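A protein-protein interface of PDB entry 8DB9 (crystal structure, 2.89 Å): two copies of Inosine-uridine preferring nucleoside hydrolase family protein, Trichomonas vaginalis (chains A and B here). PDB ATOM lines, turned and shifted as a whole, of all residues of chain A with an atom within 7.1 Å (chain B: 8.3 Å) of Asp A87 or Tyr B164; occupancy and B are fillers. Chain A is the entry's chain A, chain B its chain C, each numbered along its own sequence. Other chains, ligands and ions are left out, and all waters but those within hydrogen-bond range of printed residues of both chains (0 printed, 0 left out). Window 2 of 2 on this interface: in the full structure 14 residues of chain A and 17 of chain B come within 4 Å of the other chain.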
ATOM      1  N   ILE A  11      -1.820 -18.356  -9.642  1.00  0.00           N
ATOM      2  CA  ILE A  11      -1.163 -18.195  -8.345  1.00  0.00           C
ATOM      3  C   ILE A  11      -1.906 -18.944  -7.227  1.00  0.00           C
ATOM      4  O   ILE A  11      -1.294 -19.670  -6.416  1.00  0.00           O
ATOM      5  CB  ILE A  11      -0.997 -16.692  -8.057  1.00  0.00           C
ATOM      6  CG1 ILE A  11       0.051 -16.102  -9.020  1.00  0.00           C
ATOM      7  CG2 ILE A  11      -0.663 -16.423  -6.586  1.00  0.00           C
ATOM      8  CD1 ILE A  11      -0.482 -14.983  -9.877  1.00  0.00           C
ATOM      9  N   ARG A  49       6.413 -26.534 -11.860  1.00  0.00           N
ATOM     10  CA  ARG A  49       7.113 -25.616 -10.965  1.00  0.00           C
ATOM     11  C   ARG A  49       6.732 -25.849  -9.515  1.00  0.00           C
ATOM     12  O   ARG A  49       7.605 -25.879  -8.638  1.00  0.00           O
ATOM     13  CB  ARG A  49       6.824 -24.164 -11.337  1.00  0.00           C
ATOM     14  CG  ARG A  49       7.535 -23.688 -12.559  1.00  0.00           C
ATOM     15  CD  ARG A  49       6.803 -22.529 -13.215  1.00  0.00           C
ATOM     16  NE  ARG A  49       7.721 -21.577 -13.836  1.00  0.00           N
ATOM     17  CZ  ARG A  49       7.346 -20.455 -14.454  1.00  0.00           C
ATOM     18  NH1 ARG A  49       6.053 -20.154 -14.548  1.00  0.00           N
ATOM     19  NH2 ARG A  49       8.259 -19.647 -15.004  1.00  0.00           N
ATOM     20  N   ILE A  76      -5.988 -14.186 -18.466  1.00  0.00           N
ATOM     21  CA  ILE A  76      -5.916 -12.924 -17.726  1.00  0.00           C
ATOM     22  C   ILE A  76      -4.481 -12.551 -17.341  1.00  0.00           C
ATOM     23  O   ILE A  76      -4.128 -12.594 -16.149  1.00  0.00           O
ATOM     24  CB  ILE A  76      -6.824 -12.968 -16.486  1.00  0.00           C
ATOM     25  CG1 ILE A  76      -6.738 -14.306 -15.780  1.00  0.00           C
ATOM     26  CG2 ILE A  76      -8.256 -12.748 -16.871  1.00  0.00           C
ATOM     27  CD1 ILE A  76      -7.420 -14.249 -14.429  1.00  0.00           C
ATOM     28  N   PRO A  77      -3.617 -12.166 -18.289  1.00  0.00           N
ATOM     29  CA  PRO A  77      -2.232 -11.873 -17.912  1.00  0.00           C
ATOM     30  C   PRO A  77      -2.072 -10.587 -17.108  1.00  0.00           C
ATOM     31  O   PRO A  77      -0.982 -10.347 -16.568  1.00  0.00           O
ATOM     32  CB  PRO A  77      -1.510 -11.818 -19.266  1.00  0.00           C
ATOM     33  CG  PRO A  77      -2.550 -11.517 -20.250  1.00  0.00           C
ATOM     34  CD  PRO A  77      -3.795 -12.153 -19.753  1.00  0.00           C
ATOM     35  N   HIS A  78      -3.118  -9.768 -16.983  1.00  0.00           N
ATOM     36  CA  HIS A  78      -3.031  -8.615 -16.103  1.00  0.00           C
ATOM     37  C   HIS A  78      -3.243  -8.977 -14.649  1.00  0.00           C
ATOM     38  O   HIS A  78      -2.869  -8.199 -13.769  1.00  0.00           O
ATOM     39  CB  HIS A  78      -4.028  -7.533 -16.511  1.00  0.00           C
ATOM     40  CG  HIS A  78      -5.440  -8.007 -16.658  1.00  0.00           C
ATOM     41  ND1 HIS A  78      -6.427  -7.678 -15.755  1.00  0.00           N
ATOM     42  CD2 HIS A  78      -6.046  -8.732 -17.630  1.00  0.00           C
ATOM     43  CE1 HIS A  78      -7.575  -8.196 -16.153  1.00  0.00           C
ATOM     44  NE2 HIS A  78      -7.372  -8.838 -17.289  1.00  0.00           N
ATOM     45  N   ILE A  79      -3.817 -10.139 -14.365  1.00  0.00           N
ATOM     46  CA  ILE A  79      -4.044 -10.558 -12.991  1.00  0.00           C
ATOM     47  C   ILE A  79      -3.021 -11.595 -12.535  1.00  0.00           C
ATOM     48  O   ILE A  79      -2.529 -11.519 -11.413  1.00  0.00           O
ATOM     49  CB  ILE A  79      -5.491 -11.068 -12.814  1.00  0.00           C
ATOM     50  CG1 ILE A  79      -6.489 -10.009 -13.310  1.00  0.00           C
ATOM     51  CG2 ILE A  79      -5.768 -11.398 -11.355  1.00  0.00           C
ATOM     52  CD1 ILE A  79      -7.945 -10.309 -12.987  1.00  0.00           C
ATOM     53  N   HIS A  80      -2.649 -12.555 -13.378  1.00  0.00           N
ATOM     54  CA  HIS A  80      -1.727 -13.613 -12.967  1.00  0.00           C
ATOM     55  C   HIS A  80      -0.310 -13.463 -13.544  1.00  0.00           C
ATOM     56  O   HIS A  80       0.556 -14.300 -13.260  1.00  0.00           O
ATOM     57  CB  HIS A  80      -2.311 -14.986 -13.356  1.00  0.00           C
ATOM     58  CG  HIS A  80      -3.566 -15.354 -12.614  1.00  0.00           C
ATOM     59  ND1 HIS A  80      -3.701 -16.536 -11.916  1.00  0.00           N
ATOM     60  CD2 HIS A  80      -4.746 -14.702 -12.473  1.00  0.00           C
ATOM     61  CE1 HIS A  80      -4.907 -16.593 -11.374  1.00  0.00           C
ATOM     62  NE2 HIS A  80      -5.562 -15.494 -11.699  1.00  0.00           N
ATOM     63  N   GLY A  81      -0.043 -12.434 -14.340  1.00  0.00           N
ATOM     64  CA  GLY A  81       1.198 -12.366 -15.085  1.00  0.00           C
ATOM     65  C   GLY A  81       1.118 -13.043 -16.449  1.00  0.00           C
ATOM     66  O   GLY A  81       0.100 -13.612 -16.855  1.00  0.00           O
ATOM     67  N   GLY A  82       2.243 -12.985 -17.168  1.00  0.00           N
ATOM     68  CA  GLY A  82       2.301 -13.627 -18.469  1.00  0.00           C
ATOM     69  C   GLY A  82       2.464 -15.136 -18.384  1.00  0.00           C
ATOM     70  O   GLY A  82       1.763 -15.884 -19.068  1.00  0.00           O
ATOM     71  N   ASP A  83       3.399 -15.612 -17.553  1.00  0.00           N
ATOM     72  CA  ASP A  83       3.625 -17.058 -17.465  1.00  0.00           C
ATOM     73  C   ASP A  83       2.456 -17.811 -16.826  1.00  0.00           C
ATOM     74  O   ASP A  83       2.426 -19.053 -16.866  1.00  0.00           O
ATOM     75  CB  ASP A  83       4.925 -17.360 -16.693  1.00  0.00           C
ATOM     76  CG  ASP A  83       4.925 -16.827 -15.245  1.00  0.00           C
ATOM     77  OD1 ASP A  83       3.996 -16.109 -14.821  1.00  0.00           O
ATOM     78  OD2 ASP A  83       5.888 -17.140 -14.518  1.00  0.00           O
ATOM     79  N   GLY A  84       1.491 -17.087 -16.266  1.00  0.00           N
ATOM     80  CA  GLY A  84       0.483 -17.678 -15.438  1.00  0.00           C
ATOM     81  C   GLY A  84       0.834 -17.762 -13.972  1.00  0.00           C
ATOM     82  O   GLY A  84      -0.080 -17.877 -13.154  1.00  0.00           O
ATOM     83  N   LEU A  85       2.118 -17.690 -13.596  1.00  0.00           N
ATOM     84  CA  LEU A  85       2.524 -17.966 -12.211  1.00  0.00           C
ATOM     85  C   LEU A  85       3.233 -16.788 -11.526  1.00  0.00           C
ATOM     86  O   LEU A  85       4.108 -16.986 -10.678  1.00  0.00           O
ATOM     87  CB  LEU A  85       3.401 -19.219 -12.139  1.00  0.00           C
ATOM     88  CG  LEU A  85       3.378 -20.021 -10.827  1.00  0.00           C
ATOM     89  CD1 LEU A  85       1.983 -20.483 -10.433  1.00  0.00           C
ATOM     90  CD2 LEU A  85       4.296 -21.203 -10.894  1.00  0.00           C
ATOM     91  N   GLY A  86       2.829 -15.548 -11.827  1.00  0.00           N
ATOM     92  CA  GLY A  86       3.402 -14.383 -11.173  1.00  0.00           C
ATOM     93  C   GLY A  86       4.690 -13.892 -11.780  1.00  0.00           C
ATOM     94  O   GLY A  86       5.308 -12.977 -11.227  1.00  0.00           O
ATOM     95  N   ASP A  87       5.107 -14.484 -12.901  1.00  0.00           N
ATOM     96  CA  ASP A  87       6.337 -14.142 -13.622  1.00  0.00           C
ATOM     97  C   ASP A  87       7.559 -14.278 -12.712  1.00  0.00           C
ATOM     98  O   ASP A  87       8.337 -13.344 -12.519  1.00  0.00           O
ATOM     99  CB  ASP A  87       6.246 -12.748 -14.259  1.00  0.00           C
ATOM    100  CG  ASP A  87       5.183 -12.667 -15.367  1.00  0.00           C
ATOM    101  OD1 ASP A  87       5.125 -13.582 -16.213  1.00  0.00           O
ATOM    102  OD2 ASP A  87       4.405 -11.684 -15.404  1.00  0.00           O
ATOM    103  N   ILE A  88       7.725 -15.461 -12.160  1.00  0.00           N
ATOM    104  CA  ILE A  88       8.904 -15.774 -11.365  1.00  0.00           C
ATOM    105  C   ILE A  88       9.940 -16.451 -12.253  1.00  0.00           C
ATOM    106  O   ILE A  88       9.615 -17.205 -13.177  1.00  0.00           O
ATOM    107  CB  ILE A  88       8.550 -16.666 -10.160  1.00  0.00           C
ATOM    108  CG1 ILE A  88       8.060 -18.026 -10.667  1.00  0.00           C
ATOM    109  CG2 ILE A  88       7.537 -15.967  -9.243  1.00  0.00           C
ATOM    110  CD1 ILE A  88       8.311 -19.179  -9.699  1.00  0.00           C
ATOM    111  N   ASN A  89      11.208 -16.180 -11.968  1.00  0.00           N
ATOM    112  CA  ASN A  89      12.298 -16.751 -12.745  1.00  0.00           C
ATOM    113  C   ASN A  89      12.673 -18.122 -12.194  1.00  0.00           C
ATOM    114  O   ASN A  89      12.744 -18.317 -10.980  1.00  0.00           O
ATOM    115  CB  ASN A  89      13.512 -15.818 -12.736  1.00  0.00           C
ATOM    116  CG  ASN A  89      14.440 -16.054 -13.920  1.00  0.00           C
ATOM    117  OD1 ASN A  89      14.652 -17.195 -14.338  1.00  0.00           O
ATOM    118  ND2 ASN A  89      15.019 -14.979 -14.446  1.00  0.00           N
ATOM    119  N   GLU A 222       6.828 -14.567  -3.864  1.00  0.00           N
ATOM    120  CA  GLU A 222       6.968 -13.796  -5.096  1.00  0.00           C
ATOM    121  C   GLU A 222       5.941 -14.188  -6.152  1.00  0.00           C
ATOM    122  O   GLU A 222       5.623 -13.362  -7.019  1.00  0.00           O
ATOM    123  CB  GLU A 222       8.397 -13.883  -5.643  1.00  0.00           C
ATOM    124  CG  GLU A 222       9.353 -12.876  -4.961  1.00  0.00           C
ATOM    125  CD  GLU A 222       9.753 -11.690  -5.853  1.00  0.00           C
ATOM    126  OE1 GLU A 222      10.310 -10.705  -5.296  1.00  0.00           O
ATOM    127  OE2 GLU A 222       9.518 -11.731  -7.088  1.00  0.00           O
ATOM    128  N   THR A 223       5.373 -15.400  -6.082  1.00  0.00           N
ATOM    129  CA  THR A 223       4.226 -15.715  -6.935  1.00  0.00           C
ATOM    130  C   THR A 223       3.039 -14.816  -6.617  1.00  0.00           C
ATOM    131  O   THR A 223       2.403 -14.273  -7.525  1.00  0.00           O
ATOM    132  CB  THR A 223       3.782 -17.172  -6.791  1.00  0.00           C
ATOM    133  OG1 THR A 223       3.484 -17.467  -5.418  1.00  0.00           O
ATOM    134  CG2 THR A 223       4.836 -18.143  -7.348  1.00  0.00           C
ATOM    135  N   PRO A 226       1.747 -10.082  -7.831  1.00  0.00           N
ATOM    136  CA  PRO A 226       0.938  -9.303  -8.796  1.00  0.00           C
ATOM    137  C   PRO A 226      -0.572  -9.336  -8.596  1.00  0.00           C
ATOM    138  O   PRO A 226      -1.237  -8.301  -8.701  1.00  0.00           O
ATOM    139  CB  PRO A 226       1.289  -9.953 -10.146  1.00  0.00           C
ATOM    140  CG  PRO A 226       2.446 -10.817  -9.881  1.00  0.00           C
ATOM    141  CD  PRO A 226       2.338 -11.257  -8.485  1.00  0.00           C
ATOM    142  N   ALA B 154       3.443   0.528 -19.297  1.00  0.00           N
ATOM    143  CA  ALA B 154       3.308  -0.012 -17.946  1.00  0.00           C
ATOM    144  C   ALA B 154       4.706   0.023 -17.336  1.00  0.00           C
ATOM    145  O   ALA B 154       5.474  -0.943 -17.425  1.00  0.00           O
ATOM    146  CB  ALA B 154       2.706  -1.408 -17.933  1.00  0.00           C
ATOM    147  N   ASN B 156       7.174  -0.782 -15.192  1.00  0.00           N
ATOM    148  CA  ASN B 156       7.489  -1.800 -14.195  1.00  0.00           C
ATOM    149  C   ASN B 156       8.466  -1.243 -13.169  1.00  0.00           C
ATOM    150  O   ASN B 156       9.682  -1.219 -13.396  1.00  0.00           O
ATOM    151  CB  ASN B 156       8.086  -3.020 -14.880  1.00  0.00           C
ATOM    152  CG  ASN B 156       8.251  -4.187 -13.937  1.00  0.00           C
ATOM    153  OD1 ASN B 156       7.388  -4.444 -13.097  1.00  0.00           O
ATOM    154  ND2 ASN B 156       9.353  -4.915 -14.076  1.00  0.00           N
ATOM    155  N   ASN B 160       3.744  -3.646  -7.600  1.00  0.00           N
ATOM    156  CA  ASN B 160       3.825  -5.001  -8.128  1.00  0.00           C
ATOM    157  C   ASN B 160       2.900  -5.272  -9.316  1.00  0.00           C
ATOM    158  O   ASN B 160       2.726  -6.442  -9.689  1.00  0.00           O
ATOM    159  CB  ASN B 160       3.534  -6.023  -7.017  1.00  0.00           C
ATOM    160  CG  ASN B 160       4.608  -6.047  -5.936  1.00  0.00           C
ATOM    161  OD1 ASN B 160       5.771  -5.698  -6.169  1.00  0.00           O
ATOM    162  ND2 ASN B 160       4.211  -6.427  -4.738  1.00  0.00           N
ATOM    163  N   ILE B 161       2.294  -4.235  -9.905  1.00  0.00           N
ATOM    164  CA  ILE B 161       1.509  -4.391 -11.129  1.00  0.00           C
ATOM    165  C   ILE B 161       2.370  -5.007 -12.228  1.00  0.00           C
ATOM    166  O   ILE B 161       3.521  -4.599 -12.442  1.00  0.00           O
ATOM    167  CB  ILE B 161       0.966  -3.025 -11.584  1.00  0.00           C
ATOM    168  CG1 ILE B 161       0.450  -2.227 -10.401  1.00  0.00           C
ATOM    169  CG2 ILE B 161      -0.152  -3.172 -12.632  1.00  0.00           C
ATOM    170  CD1 ILE B 161      -0.901  -2.669  -9.923  1.00  0.00           C
ATOM    171  N   THR B 162       1.803  -5.975 -12.968  1.00  0.00           N
ATOM    172  CA  THR B 162       2.629  -6.566 -14.024  1.00  0.00           C
ATOM    173  C   THR B 162       2.454  -5.802 -15.321  1.00  0.00           C
ATOM    174  O   THR B 162       1.321  -5.468 -15.680  1.00  0.00           O
ATOM    175  CB  THR B 162       2.260  -8.019 -14.271  1.00  0.00           C
ATOM    176  OG1 THR B 162       0.836  -8.169 -14.147  1.00  0.00           O
ATOM    177  CG2 THR B 162       3.003  -8.936 -13.312  1.00  0.00           C
ATOM    178  N   PRO B 163       3.533  -5.575 -16.072  1.00  0.00           N
ATOM    179  CA  PRO B 163       3.411  -4.852 -17.341  1.00  0.00           C
ATOM    180  C   PRO B 163       2.745  -5.661 -18.442  1.00  0.00           C
ATOM    181  O   PRO B 163       2.532  -5.123 -19.535  1.00  0.00           O
ATOM    182  CB  PRO B 163       4.872  -4.526 -17.695  1.00  0.00           C
ATOM    183  CG  PRO B 163       5.661  -4.890 -16.487  1.00  0.00           C
ATOM    184  CD  PRO B 163       4.920  -5.968 -15.808  1.00  0.00           C
ATOM    185  N   TYR B 164       2.416  -6.932 -18.182  1.00  0.00           N
ATOM    186  CA  TYR B 164       1.719  -7.780 -19.143  1.00  0.00           C
ATOM    187  C   TYR B 164       0.222  -7.490 -19.234  1.00  0.00           C
ATOM    188  O   TYR B 164      -0.449  -8.053 -20.108  1.00  0.00           O
ATOM    189  CB  TYR B 164       1.935  -9.244 -18.792  1.00  0.00           C
ATOM    190  CG  TYR B 164       3.321  -9.664 -19.092  1.00  0.00           C
ATOM    191  CD1 TYR B 164       4.093  -8.951 -19.992  1.00  0.00           C
ATOM    192  CD2 TYR B 164       3.892 -10.734 -18.450  1.00  0.00           C
ATOM    193  CE1 TYR B 164       5.411  -9.314 -20.271  1.00  0.00           C
ATOM    194  CE2 TYR B 164       5.207 -11.120 -18.726  1.00  0.00           C
ATOM    195  CZ  TYR B 164       5.961 -10.404 -19.633  1.00  0.00           C
ATOM    196  OH  TYR B 164       7.259 -10.797 -19.896  1.00  0.00           O
ATOM    197  N   GLY B 165      -0.325  -6.636 -18.363  1.00  0.00           N
ATOM    198  CA  GLY B 165      -1.676  -6.163 -18.588  1.00  0.00           C
ATOM    199  C   GLY B 165      -1.748  -4.991 -19.533  1.00  0.00           C
ATOM    200  O   GLY B 165      -2.829  -4.683 -20.052  1.00  0.00           O
ATOM    201  N   GLU B 166      -0.618  -4.321 -19.737  1.00  0.00           N
ATOM    202  CA  GLU B 166      -0.489  -3.279 -20.740  1.00  0.00           C
ATOM    203  C   GLU B 166      -0.781  -3.855 -22.121  1.00  0.00           C
ATOM    204  O   GLU B 166      -0.474  -5.013 -22.412  1.00  0.00           O
ATOM    205  CB  GLU B 166       0.923  -2.693 -20.691  1.00  0.00           C
ATOM    206  CG  GLU B 166       1.030  -1.297 -21.249  1.00  0.00           C
ATOM    207  CD  GLU B 166       1.129  -1.283 -22.761  1.00  0.00           C
ATOM    208  OE1 GLU B 166       1.845  -2.130 -23.347  1.00  0.00           O
ATOM    209  OE2 GLU B 166       0.443  -0.441 -23.364  1.00  0.00           O
ATOM    210  N   PHE B 167      -1.383  -3.039 -22.983  1.00  0.00           N
ATOM    211  CA  PHE B 167      -1.910  -3.565 -24.236  1.00  0.00           C
ATOM    212  C   PHE B 167      -1.569  -2.634 -25.382  1.00  0.00           C
ATOM    213  O   PHE B 167      -1.139  -3.075 -26.456  1.00  0.00           O
ATOM    214  CB  PHE B 167      -3.442  -3.757 -24.142  1.00  0.00           C
ATOM    215  CG  PHE B 167      -4.136  -3.976 -25.486  1.00  0.00           C
ATOM    216  CD1 PHE B 167      -4.207  -5.241 -26.052  1.00  0.00           C
ATOM    217  CD2 PHE B 167      -4.720  -2.914 -26.172  1.00  0.00           C
ATOM    218  CE1 PHE B 167      -4.829  -5.435 -27.263  1.00  0.00           C
ATOM    219  CE2 PHE B 167      -5.343  -3.108 -27.386  1.00  0.00           C
ATOM    220  CZ  PHE B 167      -5.398  -4.367 -27.925  1.00  0.00           C
ATOM    221  N   ARG B 170       2.254  -2.864 -26.350  1.00  0.00           N
ATOM    222  CA  ARG B 170       2.647  -4.190 -26.818  1.00  0.00           C
ATOM    223  C   ARG B 170       1.932  -4.585 -28.107  1.00  0.00           C
ATOM    224  O   ARG B 170       2.481  -5.349 -28.912  1.00  0.00           O
ATOM    225  CB  ARG B 170       2.380  -5.227 -25.737  1.00  0.00           C
ATOM    226  CG  ARG B 170       2.972  -6.605 -26.026  1.00  0.00           C
ATOM    227  CD  ARG B 170       2.794  -7.526 -24.836  1.00  0.00           C
ATOM    228  NE  ARG B 170       3.652  -7.127 -23.733  1.00  0.00           N
ATOM    229  CZ  ARG B 170       3.269  -6.359 -22.716  1.00  0.00           C
ATOM    230  NH1 ARG B 170       2.028  -5.908 -22.660  1.00  0.00           N
ATOM    231  NH2 ARG B 170       4.135  -6.041 -21.754  1.00  0.00           N
ATOM    232  N   TRP B 193      -0.870   1.861 -17.779  1.00  0.00           N
ATOM    233  CA  TRP B 193      -1.813   0.839 -17.359  1.00  0.00           C
ATOM    234  C   TRP B 193      -1.700   0.607 -15.875  1.00  0.00           C
ATOM    235  O   TRP B 193      -2.695   0.328 -15.207  1.00  0.00           O
ATOM    236  CB  TRP B 193      -1.571  -0.449 -18.133  1.00  0.00           C
ATOM    237  CG  TRP B 193      -2.164  -1.684 -17.542  1.00  0.00           C
ATOM    238  CD1 TRP B 193      -1.488  -2.792 -17.130  1.00  0.00           C
ATOM    239  CD2 TRP B 193      -3.549  -1.960 -17.335  1.00  0.00           C
ATOM    240  NE1 TRP B 193      -2.360  -3.741 -16.672  1.00  0.00           N
ATOM    241  CE2 TRP B 193      -3.636  -3.258 -16.788  1.00  0.00           C
ATOM    242  CE3 TRP B 193      -4.730  -1.240 -17.557  1.00  0.00           C
ATOM    243  CZ2 TRP B 193      -4.855  -3.852 -16.465  1.00  0.00           C
ATOM    244  CZ3 TRP B 193      -5.938  -1.829 -17.226  1.00  0.00           C
ATOM    245  CH2 TRP B 193      -5.989  -3.121 -16.686  1.00  0.00           C
ATOM    246  N   THR B 194      -0.504   0.744 -15.343  1.00  0.00           N
ATOM    247  CA  THR B 194      -0.333   0.675 -13.905  1.00  0.00           C
ATOM    248  C   THR B 194      -1.041   1.847 -13.209  1.00  0.00           C
ATOM    249  O   THR B 194      -1.680   1.659 -12.164  1.00  0.00           O
ATOM    250  CB  THR B 194       1.169   0.602 -13.611  1.00  0.00           C
ATOM    251  OG1 THR B 194       1.814   1.780 -14.091  1.00  0.00           O
ATOM    252  CG2 THR B 194       1.773  -0.581 -14.371  1.00  0.00           C
ATOM    253  N   GLU B 268      13.102 -10.754 -24.932  1.00  0.00           N
ATOM    254  CA  GLU B 268      12.071 -11.396 -24.126  1.00  0.00           C
ATOM    255  C   GLU B 268      10.840 -10.524 -23.922  1.00  0.00           C
ATOM    256  O   GLU B 268       9.714 -10.961 -24.156  1.00  0.00           O
ATOM    257  CB  GLU B 268      12.640 -11.818 -22.768  1.00  0.00           C
ATOM    258  CG  GLU B 268      13.731 -10.901 -22.239  1.00  0.00           C
ATOM    259  CD  GLU B 268      15.050 -11.086 -22.963  1.00  0.00           C
ATOM    260  OE1 GLU B 268      15.369 -10.255 -23.839  1.00  0.00           O
ATOM    261  OE2 GLU B 268      15.766 -12.062 -22.657  1.00  0.00           O
ATOM    262  N   LYS B 269      11.060  -9.291 -23.483  1.00  0.00           N
ATOM    263  CA  LYS B 269       9.958  -8.373 -23.233  1.00  0.00           C
ATOM    264  C   LYS B 269       9.839  -7.280 -24.289  1.00  0.00           C
ATOM    265  O   LYS B 269      10.121  -6.114 -24.012  1.00  0.00           O
ATOM    266  CB  LYS B 269      10.099  -7.741 -21.845  1.00  0.00           C
ATOM    267  CG  LYS B 269      11.467  -7.136 -21.575  1.00  0.00           C
ATOM    268  CD  LYS B 269      12.359  -8.104 -20.814  1.00  0.00           C
ATOM    269  CE  LYS B 269      13.805  -7.634 -20.810  1.00  0.00           C
ATOM    270  NZ  LYS B 269      14.683  -8.544 -20.023  1.00  0.00           N
ATOM    271  N   LEU B 270       9.429  -7.655 -25.498  1.00  0.00           N
ATOM    272  CA  LEU B 270       9.255  -6.679 -26.553  1.00  0.00           C
ATOM    273  C   LEU B 270       8.467  -5.434 -26.215  1.00  0.00           C
ATOM    274  O   LEU B 270       8.983  -4.338 -26.307  1.00  0.00           O
ATOM    275  CB  LEU B 270       8.682  -7.332 -27.788  1.00  0.00           C
ATOM    276  CG  LEU B 270       9.196  -6.819 -29.129  1.00  0.00           C
ATOM    277  CD1 LEU B 270       9.274  -7.903 -30.172  1.00  0.00           C
ATOM    278  CD2 LEU B 270       8.341  -5.694 -29.643  1.00  0.00           C
ATOM    279  N   GLY B 271       7.207  -5.566 -25.854  1.00  0.00           N
ATOM    280  CA  GLY B 271       6.422  -4.386 -25.539  1.00  0.00           C
ATOM    281  C   GLY B 271       6.549  -3.838 -24.135  1.00  0.00           C
ATOM    282  O   GLY B 271       5.583  -3.623 -23.427  1.00  0.00           O
ATOM    283  N   MET B 272       7.763  -3.588 -23.721  1.00  0.00           N
ATOM    284  CA  MET B 272       7.991  -3.063 -22.385  1.00  0.00           C
ATOM    285  C   MET B 272       8.592  -1.663 -22.481  1.00  0.00           C
ATOM    286  O   MET B 272       8.990  -1.202 -23.551  1.00  0.00           O
ATOM    287  CB  MET B 272       8.856  -4.019 -21.556  1.00  0.00           C
ATOM    288  CG  MET B 272       8.353  -5.471 -21.550  1.00  0.00           C
ATOM    289  SD  MET B 272       7.209  -5.914 -20.223  1.00  0.00           S
ATOM    290  CE  MET B 272       8.248  -5.543 -18.796  1.00  0.00           C
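The side-chain carboxylate (OD1) of Asp A83 is in hydrogen-bond range of the backbone NH (N) of Asp A87, 2.7 Å away.
OD2 of Asp A87 lies within hydrogen-bond range of N of Gly A82.
Among the printed residues, merely in contact across the chains: Pro A77 with Thr B162, Pro A77 with Tyr B164, His A78 with Thr B162, His A78 with Gly B165, His A78 with Trp B193, Gly A82 with Tyr B164, Asp A87 with Thr B162, Asp A87 with Tyr B164, Pro A226 with Asn B160 and Pro A226 with Thr B162.
Of the printed residues of chain B, His A78 touches Thr B162, Gly B165 and Trp B193.
Ile A79 touches none of the printed residues of chain B.
Asp A87 touches two residues of chain B.
Ile A88 touches none of the printed residues of chain B.
Of the printed residues of chain B, Pro A226 touches Asn B160 and Thr B162.
Printed residues of chain A within 4 Å of Thr B162: Pro A77, His A78, Asp A87 and Pro A226.
Of the printed residues of chain A, Gly B165 touches His A78.
Of the 19 printed residues of chain A, 5 touch a printed residue of chain B.
Printed residues of chain A that touch a printed residue of chain B: Pro A77, His A78, Gly A82, Asp A87 and Pro A226.
Printed residues of chain B that touch a printed residue of chain A: Asn B160, Thr B162, Tyr B164, Gly B165 and Trp B193.
Hydrophobic or aromatic side chains of chain B that line the printed part of chain A: Tyr B164 and Trp B193.
Among the printed residues, 10 pairs touch across the chains.
No position is printed for both chains.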
